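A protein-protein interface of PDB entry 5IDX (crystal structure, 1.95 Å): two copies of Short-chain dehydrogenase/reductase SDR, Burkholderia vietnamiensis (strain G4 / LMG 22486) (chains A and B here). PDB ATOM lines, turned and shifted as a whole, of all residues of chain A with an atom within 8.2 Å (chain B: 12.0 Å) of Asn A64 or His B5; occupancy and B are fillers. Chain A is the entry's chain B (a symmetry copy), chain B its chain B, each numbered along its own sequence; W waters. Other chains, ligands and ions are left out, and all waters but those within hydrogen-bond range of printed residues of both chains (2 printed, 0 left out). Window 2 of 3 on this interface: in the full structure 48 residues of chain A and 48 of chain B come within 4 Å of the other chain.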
ATOM      1  N   GLY A  15       7.112  -4.081  16.739  1.00  0.00           N
ATOM      2  CA  GLY A  15       7.922  -3.047  17.348  1.00  0.00           C
ATOM      3  C   GLY A  15       7.192  -2.124  18.301  1.00  0.00           C
ATOM      4  O   GLY A  15       7.839  -1.282  18.939  1.00  0.00           O
ATOM      5  N   ALA A  36       2.736 -11.017  21.078  1.00  0.00           N
ATOM      6  CA  ALA A  36       4.135 -11.346  20.821  1.00  0.00           C
ATOM      7  C   ALA A  36       4.316 -11.940  19.425  1.00  0.00           C
ATOM      8  O   ALA A  36       5.316 -11.663  18.746  1.00  0.00           O
ATOM      9  CB  ALA A  36       4.654 -12.303  21.896  1.00  0.00           C
ATOM     10  N   ALA A  37       3.350 -12.745  18.969  1.00  0.00           N
ATOM     11  CA  ALA A  37       3.435 -13.294  17.617  1.00  0.00           C
ATOM     12  C   ALA A  37       3.294 -12.219  16.545  1.00  0.00           C
ATOM     13  O   ALA A  37       3.643 -12.465  15.384  1.00  0.00           O
ATOM     14  CB  ALA A  37       2.373 -14.380  17.418  1.00  0.00           C
ATOM     15  N   GLU A  38       2.792 -11.040  16.896  1.00  0.00           N
ATOM     16  CA  GLU A  38       2.721  -9.928  15.960  1.00  0.00           C
ATOM     17  C   GLU A  38       3.919  -8.996  16.066  1.00  0.00           C
ATOM     18  O   GLU A  38       3.905  -7.925  15.452  1.00  0.00           O
ATOM     19  CB  GLU A  38       1.429  -9.137  16.174  1.00  0.00           C
ATOM     20  CG  GLU A  38       0.180  -9.954  15.933  1.00  0.00           C
ATOM     21  CD  GLU A  38       0.111 -10.511  14.525  1.00  0.00           C
ATOM     22  OE1 GLU A  38       0.437  -9.770  13.572  1.00  0.00           O
ATOM     23  OE2 GLU A  38      -0.255 -11.697  14.374  1.00  0.00           O
ATOM     24  N   GLY A  39       4.950  -9.372  16.829  1.00  0.00           N
ATOM     25  CA  GLY A  39       6.131  -8.540  16.976  1.00  0.00           C
ATOM     26  C   GLY A  39       6.034  -7.462  18.036  1.00  0.00           C
ATOM     27  O   GLY A  39       6.879  -6.557  18.060  1.00  0.00           O
ATOM     28  N   VAL A  40       5.045  -7.533  18.917  1.00  0.00           N
ATOM     29  CA  VAL A  40       4.845  -6.530  19.955  1.00  0.00           C
ATOM     30  C   VAL A  40       5.690  -6.900  21.167  1.00  0.00           C
ATOM     31  O   VAL A  40       5.572  -8.010  21.702  1.00  0.00           O
ATOM     32  CB  VAL A  40       3.360  -6.423  20.339  1.00  0.00           C
ATOM     33  CG1 VAL A  40       3.161  -5.362  21.435  1.00  0.00           C
ATOM     34  CG2 VAL A  40       2.522  -6.130  19.103  1.00  0.00           C
ATOM     35  N   ASN A  41       6.536  -5.969  21.604  1.00  0.00           N
ATOM     36  CA  ASN A  41       7.292  -6.171  22.831  1.00  0.00           C
ATOM     37  C   ASN A  41       6.363  -6.034  24.028  1.00  0.00           C
ATOM     38  O   ASN A  41       5.404  -5.257  24.008  1.00  0.00           O
ATOM     39  CB  ASN A  41       8.441  -5.165  22.925  1.00  0.00           C
ATOM     40  CG  ASN A  41       9.430  -5.307  21.779  1.00  0.00           C
ATOM     41  OD1 ASN A  41       9.941  -6.393  21.530  1.00  0.00           O
ATOM     42  ND2 ASN A  41       9.685  -4.212  21.061  1.00  0.00           N
ATOM     43  N   ILE A  59       7.349 -17.305  26.832  1.00  0.00           N
ATOM     44  CA  ILE A  59       7.016 -16.415  25.722  1.00  0.00           C
ATOM     45  C   ILE A  59       8.276 -16.019  24.962  1.00  0.00           C
ATOM     46  O   ILE A  59       8.282 -15.985  23.724  1.00  0.00           O
ATOM     47  CB  ILE A  59       6.239 -15.182  26.225  1.00  0.00           C
ATOM     48  CG1 ILE A  59       4.904 -15.619  26.825  1.00  0.00           C
ATOM     49  CG2 ILE A  59       5.988 -14.198  25.076  1.00  0.00           C
ATOM     50  CD1 ILE A  59       4.053 -14.466  27.372  1.00  0.00           C
ATOM     51  N   ARG A  60       9.371 -15.744  25.689  1.00  0.00           N
ATOM     52  CA  ARG A  60      10.635 -15.397  25.044  1.00  0.00           C
ATOM     53  C   ARG A  60      11.099 -16.492  24.101  1.00  0.00           C
ATOM     54  O   ARG A  60      11.608 -16.206  23.011  1.00  0.00           O
ATOM     55  CB  ARG A  60      11.726 -15.138  26.088  1.00  0.00           C
ATOM     56  CG  ARG A  60      11.557 -13.855  26.864  1.00  0.00           C
ATOM     57  CD  ARG A  60      12.747 -13.580  27.809  1.00  0.00           C
ATOM     58  NE  ARG A  60      12.367 -12.540  28.759  1.00  0.00           N
ATOM     59  CZ  ARG A  60      12.196 -12.736  30.062  1.00  0.00           C
ATOM     60  NH1 ARG A  60      12.424 -13.930  30.596  1.00  0.00           N
ATOM     61  NH2 ARG A  60      11.829 -11.725  30.835  1.00  0.00           N
ATOM     62  N   ALA A  61      10.963 -17.754  24.520  1.00  0.00           N
ATOM     63  CA  ALA A  61      11.387 -18.868  23.683  1.00  0.00           C
ATOM     64  C   ALA A  61      10.507 -19.013  22.453  1.00  0.00           C
ATOM     65  O   ALA A  61      10.999 -19.389  21.383  1.00  0.00           O
ATOM     66  CB  ALA A  61      11.378 -20.166  24.492  1.00  0.00           C
ATOM     67  N   ALA A  62       9.216 -18.705  22.583  1.00  0.00           N
ATOM     68  CA  ALA A  62       8.239 -18.937  21.530  1.00  0.00           C
ATOM     69  C   ALA A  62       8.147 -17.801  20.523  1.00  0.00           C
ATOM     70  O   ALA A  62       7.520 -17.979  19.473  1.00  0.00           O
ATOM     71  CB  ALA A  62       6.853 -19.166  22.151  1.00  0.00           C
ATOM     72  N   SER A  63       8.741 -16.645  20.809  1.00  0.00           N
ATOM     73  CA  SER A  63       8.553 -15.458  19.989  1.00  0.00           C
ATOM     74  C   SER A  63       9.900 -14.797  19.735  1.00  0.00           C
ATOM     75  O   SER A  63      10.950 -15.297  20.145  1.00  0.00           O
ATOM     76  CB  SER A  63       7.601 -14.470  20.662  1.00  0.00           C
ATOM     77  OG  SER A  63       8.250 -13.887  21.764  1.00  0.00           O
ATOM     78  N   ASN A  64       9.865 -13.658  19.046  1.00  0.00           N
ATOM     79  CA  ASN A  64      11.067 -12.892  18.730  1.00  0.00           C
ATOM     80  C   ASN A  64      11.000 -11.486  19.312  1.00  0.00           C
ATOM     81  O   ASN A  64      11.534 -10.545  18.723  1.00  0.00           O
ATOM     82  CB  ASN A  64      11.286 -12.821  17.219  1.00  0.00           C
ATOM     83  CG  ASN A  64      11.666 -14.156  16.625  1.00  0.00           C
ATOM     84  OD1 ASN A  64      11.184 -14.534  15.560  1.00  0.00           O
ATOM     85  ND2 ASN A  64      12.535 -14.882  17.316  1.00  0.00           N
ATOM     86  N   VAL A  65      10.330 -11.322  20.454  1.00  0.00           N
ATOM     87  CA  VAL A  65      10.145 -10.013  21.067  1.00  0.00           C
ATOM     88  C   VAL A  65      10.778 -10.027  22.454  1.00  0.00           C
ATOM     89  O   VAL A  65      11.093 -11.077  23.011  1.00  0.00           O
ATOM     90  CB  VAL A  65       8.660  -9.603  21.149  1.00  0.00           C
ATOM     91  CG1 VAL A  65       8.002  -9.704  19.778  1.00  0.00           C
ATOM     92  CG2 VAL A  65       7.910 -10.454  22.173  1.00  0.00           C
ATOM     93  N   SER A  66      10.959  -8.834  23.012  1.00  0.00           N
ATOM     94  CA  SER A  66      11.421  -8.706  24.383  1.00  0.00           C
ATOM     95  C   SER A  66      10.231  -8.787  25.329  1.00  0.00           C
ATOM     96  O   SER A  66       9.139  -8.296  25.027  1.00  0.00           O
ATOM     97  CB  SER A  66      12.177  -7.393  24.594  1.00  0.00           C
ATOM     98  OG  SER A  66      11.293  -6.289  24.556  1.00  0.00           O
ATOM     99  N   VAL A  67      10.446  -9.433  26.471  1.00  0.00           N
ATOM    100  CA  VAL A  67       9.418  -9.591  27.495  1.00  0.00           C
ATOM    101  C   VAL A  67      10.022  -9.132  28.813  1.00  0.00           C
ATOM    102  O   VAL A  67      11.083  -9.630  29.217  1.00  0.00           O
ATOM    103  CB  VAL A  67       8.932 -11.043  27.610  1.00  0.00           C
ATOM    104  CG1 VAL A  67       7.796 -11.155  28.620  1.00  0.00           C
ATOM    105  CG2 VAL A  67       8.531 -11.594  26.235  1.00  0.00           C
ATOM    106  N   HIS B   5      10.573 -12.787  10.185  1.00  0.00           N
ATOM    107  CA  HIS B   5      10.871 -12.978  11.599  1.00  0.00           C
ATOM    108  C   HIS B   5       9.601 -13.283  12.406  1.00  0.00           C
ATOM    109  O   HIS B   5       9.479 -14.368  12.971  1.00  0.00           O
ATOM    110  CB  HIS B   5      11.583 -11.746  12.164  1.00  0.00           C
ATOM    111  N   HIS B   6       8.657 -12.340  12.459  1.00  0.00           N
ATOM    112  CA  HIS B   6       7.428 -12.551  13.220  1.00  0.00           C
ATOM    113  C   HIS B   6       6.426 -13.381  12.426  1.00  0.00           C
ATOM    114  O   HIS B   6       6.335 -13.282  11.196  1.00  0.00           O
ATOM    115  CB  HIS B   6       6.784 -11.219  13.624  1.00  0.00           C
ATOM    116  CG  HIS B   6       7.724 -10.280  14.306  1.00  0.00           C
ATOM    117  ND1 HIS B   6       8.400 -10.614  15.460  1.00  0.00           N
ATOM    118  CD2 HIS B   6       8.114  -9.022  13.991  1.00  0.00           C
ATOM    119  CE1 HIS B   6       9.164  -9.600  15.831  1.00  0.00           C
ATOM    120  NE2 HIS B   6       9.008  -8.620  14.957  1.00  0.00           N
ATOM    121  N   HIS B   7       5.650 -14.187  13.159  1.00  0.00           N
ATOM    122  CA  HIS B   7       4.752 -15.157  12.538  1.00  0.00           C
ATOM    123  C   HIS B   7       3.627 -14.471  11.765  1.00  0.00           C
ATOM    124  O   HIS B   7       3.387 -14.791  10.594  1.00  0.00           O
ATOM    125  CB  HIS B   7       4.193 -16.100  13.611  1.00  0.00           C
ATOM    126  CG  HIS B   7       3.313 -17.189  13.073  1.00  0.00           C
ATOM    127  ND1 HIS B   7       2.095 -17.507  13.636  1.00  0.00           N
ATOM    128  CD2 HIS B   7       3.474 -18.033  12.025  1.00  0.00           C
ATOM    129  CE1 HIS B   7       1.544 -18.499  12.958  1.00  0.00           C
ATOM    130  NE2 HIS B   7       2.360 -18.836  11.976  1.00  0.00           N
ATOM    131  N   HIS B   8       2.929 -13.525  12.407  1.00  0.00           N
ATOM    132  CA  HIS B   8       1.771 -12.826  11.838  1.00  0.00           C
ATOM    133  C   HIS B   8       0.594 -13.768  11.603  1.00  0.00           C
ATOM    134  O   HIS B   8       0.771 -14.977  11.418  1.00  0.00           O
ATOM    135  CB  HIS B   8       2.147 -12.096  10.546  1.00  0.00           C
ATOM    136  CG  HIS B   8       3.123 -10.986  10.761  1.00  0.00           C
ATOM    137  ND1 HIS B   8       2.804  -9.843  11.461  1.00  0.00           N
ATOM    138  CD2 HIS B   8       4.420 -10.855  10.397  1.00  0.00           C
ATOM    139  CE1 HIS B   8       3.859  -9.048  11.508  1.00  0.00           C
ATOM    140  NE2 HIS B   8       4.852  -9.638  10.867  1.00  0.00           N
ATOM    141  N   MET B   9      -0.616 -13.219  11.587  1.00  0.00           N
ATOM    142  CA  MET B   9      -1.808 -14.018  11.840  1.00  0.00           C
ATOM    143  C   MET B   9      -2.214 -14.829  10.613  1.00  0.00           C
ATOM    144  O   MET B   9      -2.629 -14.271   9.590  1.00  0.00           O
ATOM    145  CB  MET B   9      -2.953 -13.121  12.295  1.00  0.00           C
ATOM    146  CG  MET B   9      -4.106 -13.915  12.858  1.00  0.00           C
ATOM    147  SD  MET B   9      -5.404 -12.847  13.494  1.00  0.00           S
ATOM    148  CE  MET B   9      -4.752 -12.361  15.090  1.00  0.00           C
ATOM    149  N   ASP B  10      -2.143 -16.151  10.745  1.00  0.00           N
ATOM    150  CA  ASP B  10      -2.661 -17.087   9.753  1.00  0.00           C
ATOM    151  C   ASP B  10      -4.132 -17.350  10.079  1.00  0.00           C
ATOM    152  O   ASP B  10      -4.450 -17.977  11.096  1.00  0.00           O
ATOM    153  CB  ASP B  10      -1.844 -18.378   9.775  1.00  0.00           C
ATOM    154  CG  ASP B  10      -2.237 -19.359   8.665  1.00  0.00           C
ATOM    155  OD1 ASP B  10      -3.282 -19.174   8.011  1.00  0.00           O
ATOM    156  OD2 ASP B  10      -1.493 -20.342   8.461  1.00  0.00           O
HETATM  157  O   HOH W   1       9.766  -6.536  17.373  1.00  0.00           O
HETATM  158  O   HOH W   2       7.536 -12.791  17.467  1.00  0.00           O
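Of the 6 printed residues of chain B, 5 touch a printed residue of chain A. Of the 16 printed residues of chain A, 4 touch a printed residue of chain B. Among the printed residues, 8 pairs touch across the chains.
CB of His B6 touches O of Ala A37, at 3.8 Å. His B6 touches Gly A39. Asn A64 touches His B6 (O to CE1, 3.9 Å).
Water W2 lies within hydrogen-bond range of O of Ala A36 (2.8 Å), N of Asn A64 (2.9 Å) and ND1 of His B6 (3.1 Å). Water W1 bridges O of Gly A39 and NE2 of His B6.
OD1 of Asn A64 lies close to O of His B5, 3.1 Å away. The backbone carbonyl oxygen (O) of Ala A37 lies within hydrogen-bond range of the backbone NH (N) of His B7 (3.5 Å). The backbone carbonyl oxygen (O) of Ala A37 lies within hydrogen-bond range of the backbone NH (N) of His B8, at 3.2 Å. The side-chain carboxylate of Glu A38 lies within hydrogen-bond range of a ring nitrogen (ND1) of His B8, at 3.2 Å. The side-chain carboxylate (OE2) of Glu A38 lies within hydrogen-bond range of the backbone NH (N) of Met B9 (3.2 Å).
Asn A64 touches just these residues of chain B: His B5 and His B6. His B5 touches just one residue of chain A: Asn A64 (3.1 Å). No residue of chain B comes within 4 Å of Ala A36. Ala A62 touches none of the printed residues of chain B. No residue of chain B comes within 4 Å of Ser A66. Printed residues of chain A within 4 Å of His B8: Ala A37 and Glu A38. Of the printed residues of chain B, Glu A38 touches His B8 and Met B9. Of the printed residues of chain A, His B6 touches Ala A37, Gly A39 and Asn A64. Of the printed residues of chain A, His B7 touches Ala A37. Of the printed residues of chain A, Met B9 touches Glu A38 (3.2 Å). Val A67 touches none of the printed residues of chain B. The nearest residue of chain B that does not touch Asn A64 is His B7 (6.0 Å). The nearest residue of chain A that does not touch His B5 is Ala A37 (6.6 Å).
No position is printed for both chains. Of the 8 pairs that touch across the chains among the printed residues, none has its exchanged pair printed and touching as well.
The backbone carbonyl oxygen (O) of Gly A39 sits at hydrogen-bond distance from the backbone NH (N) of Gly A15 (2.8 Å).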
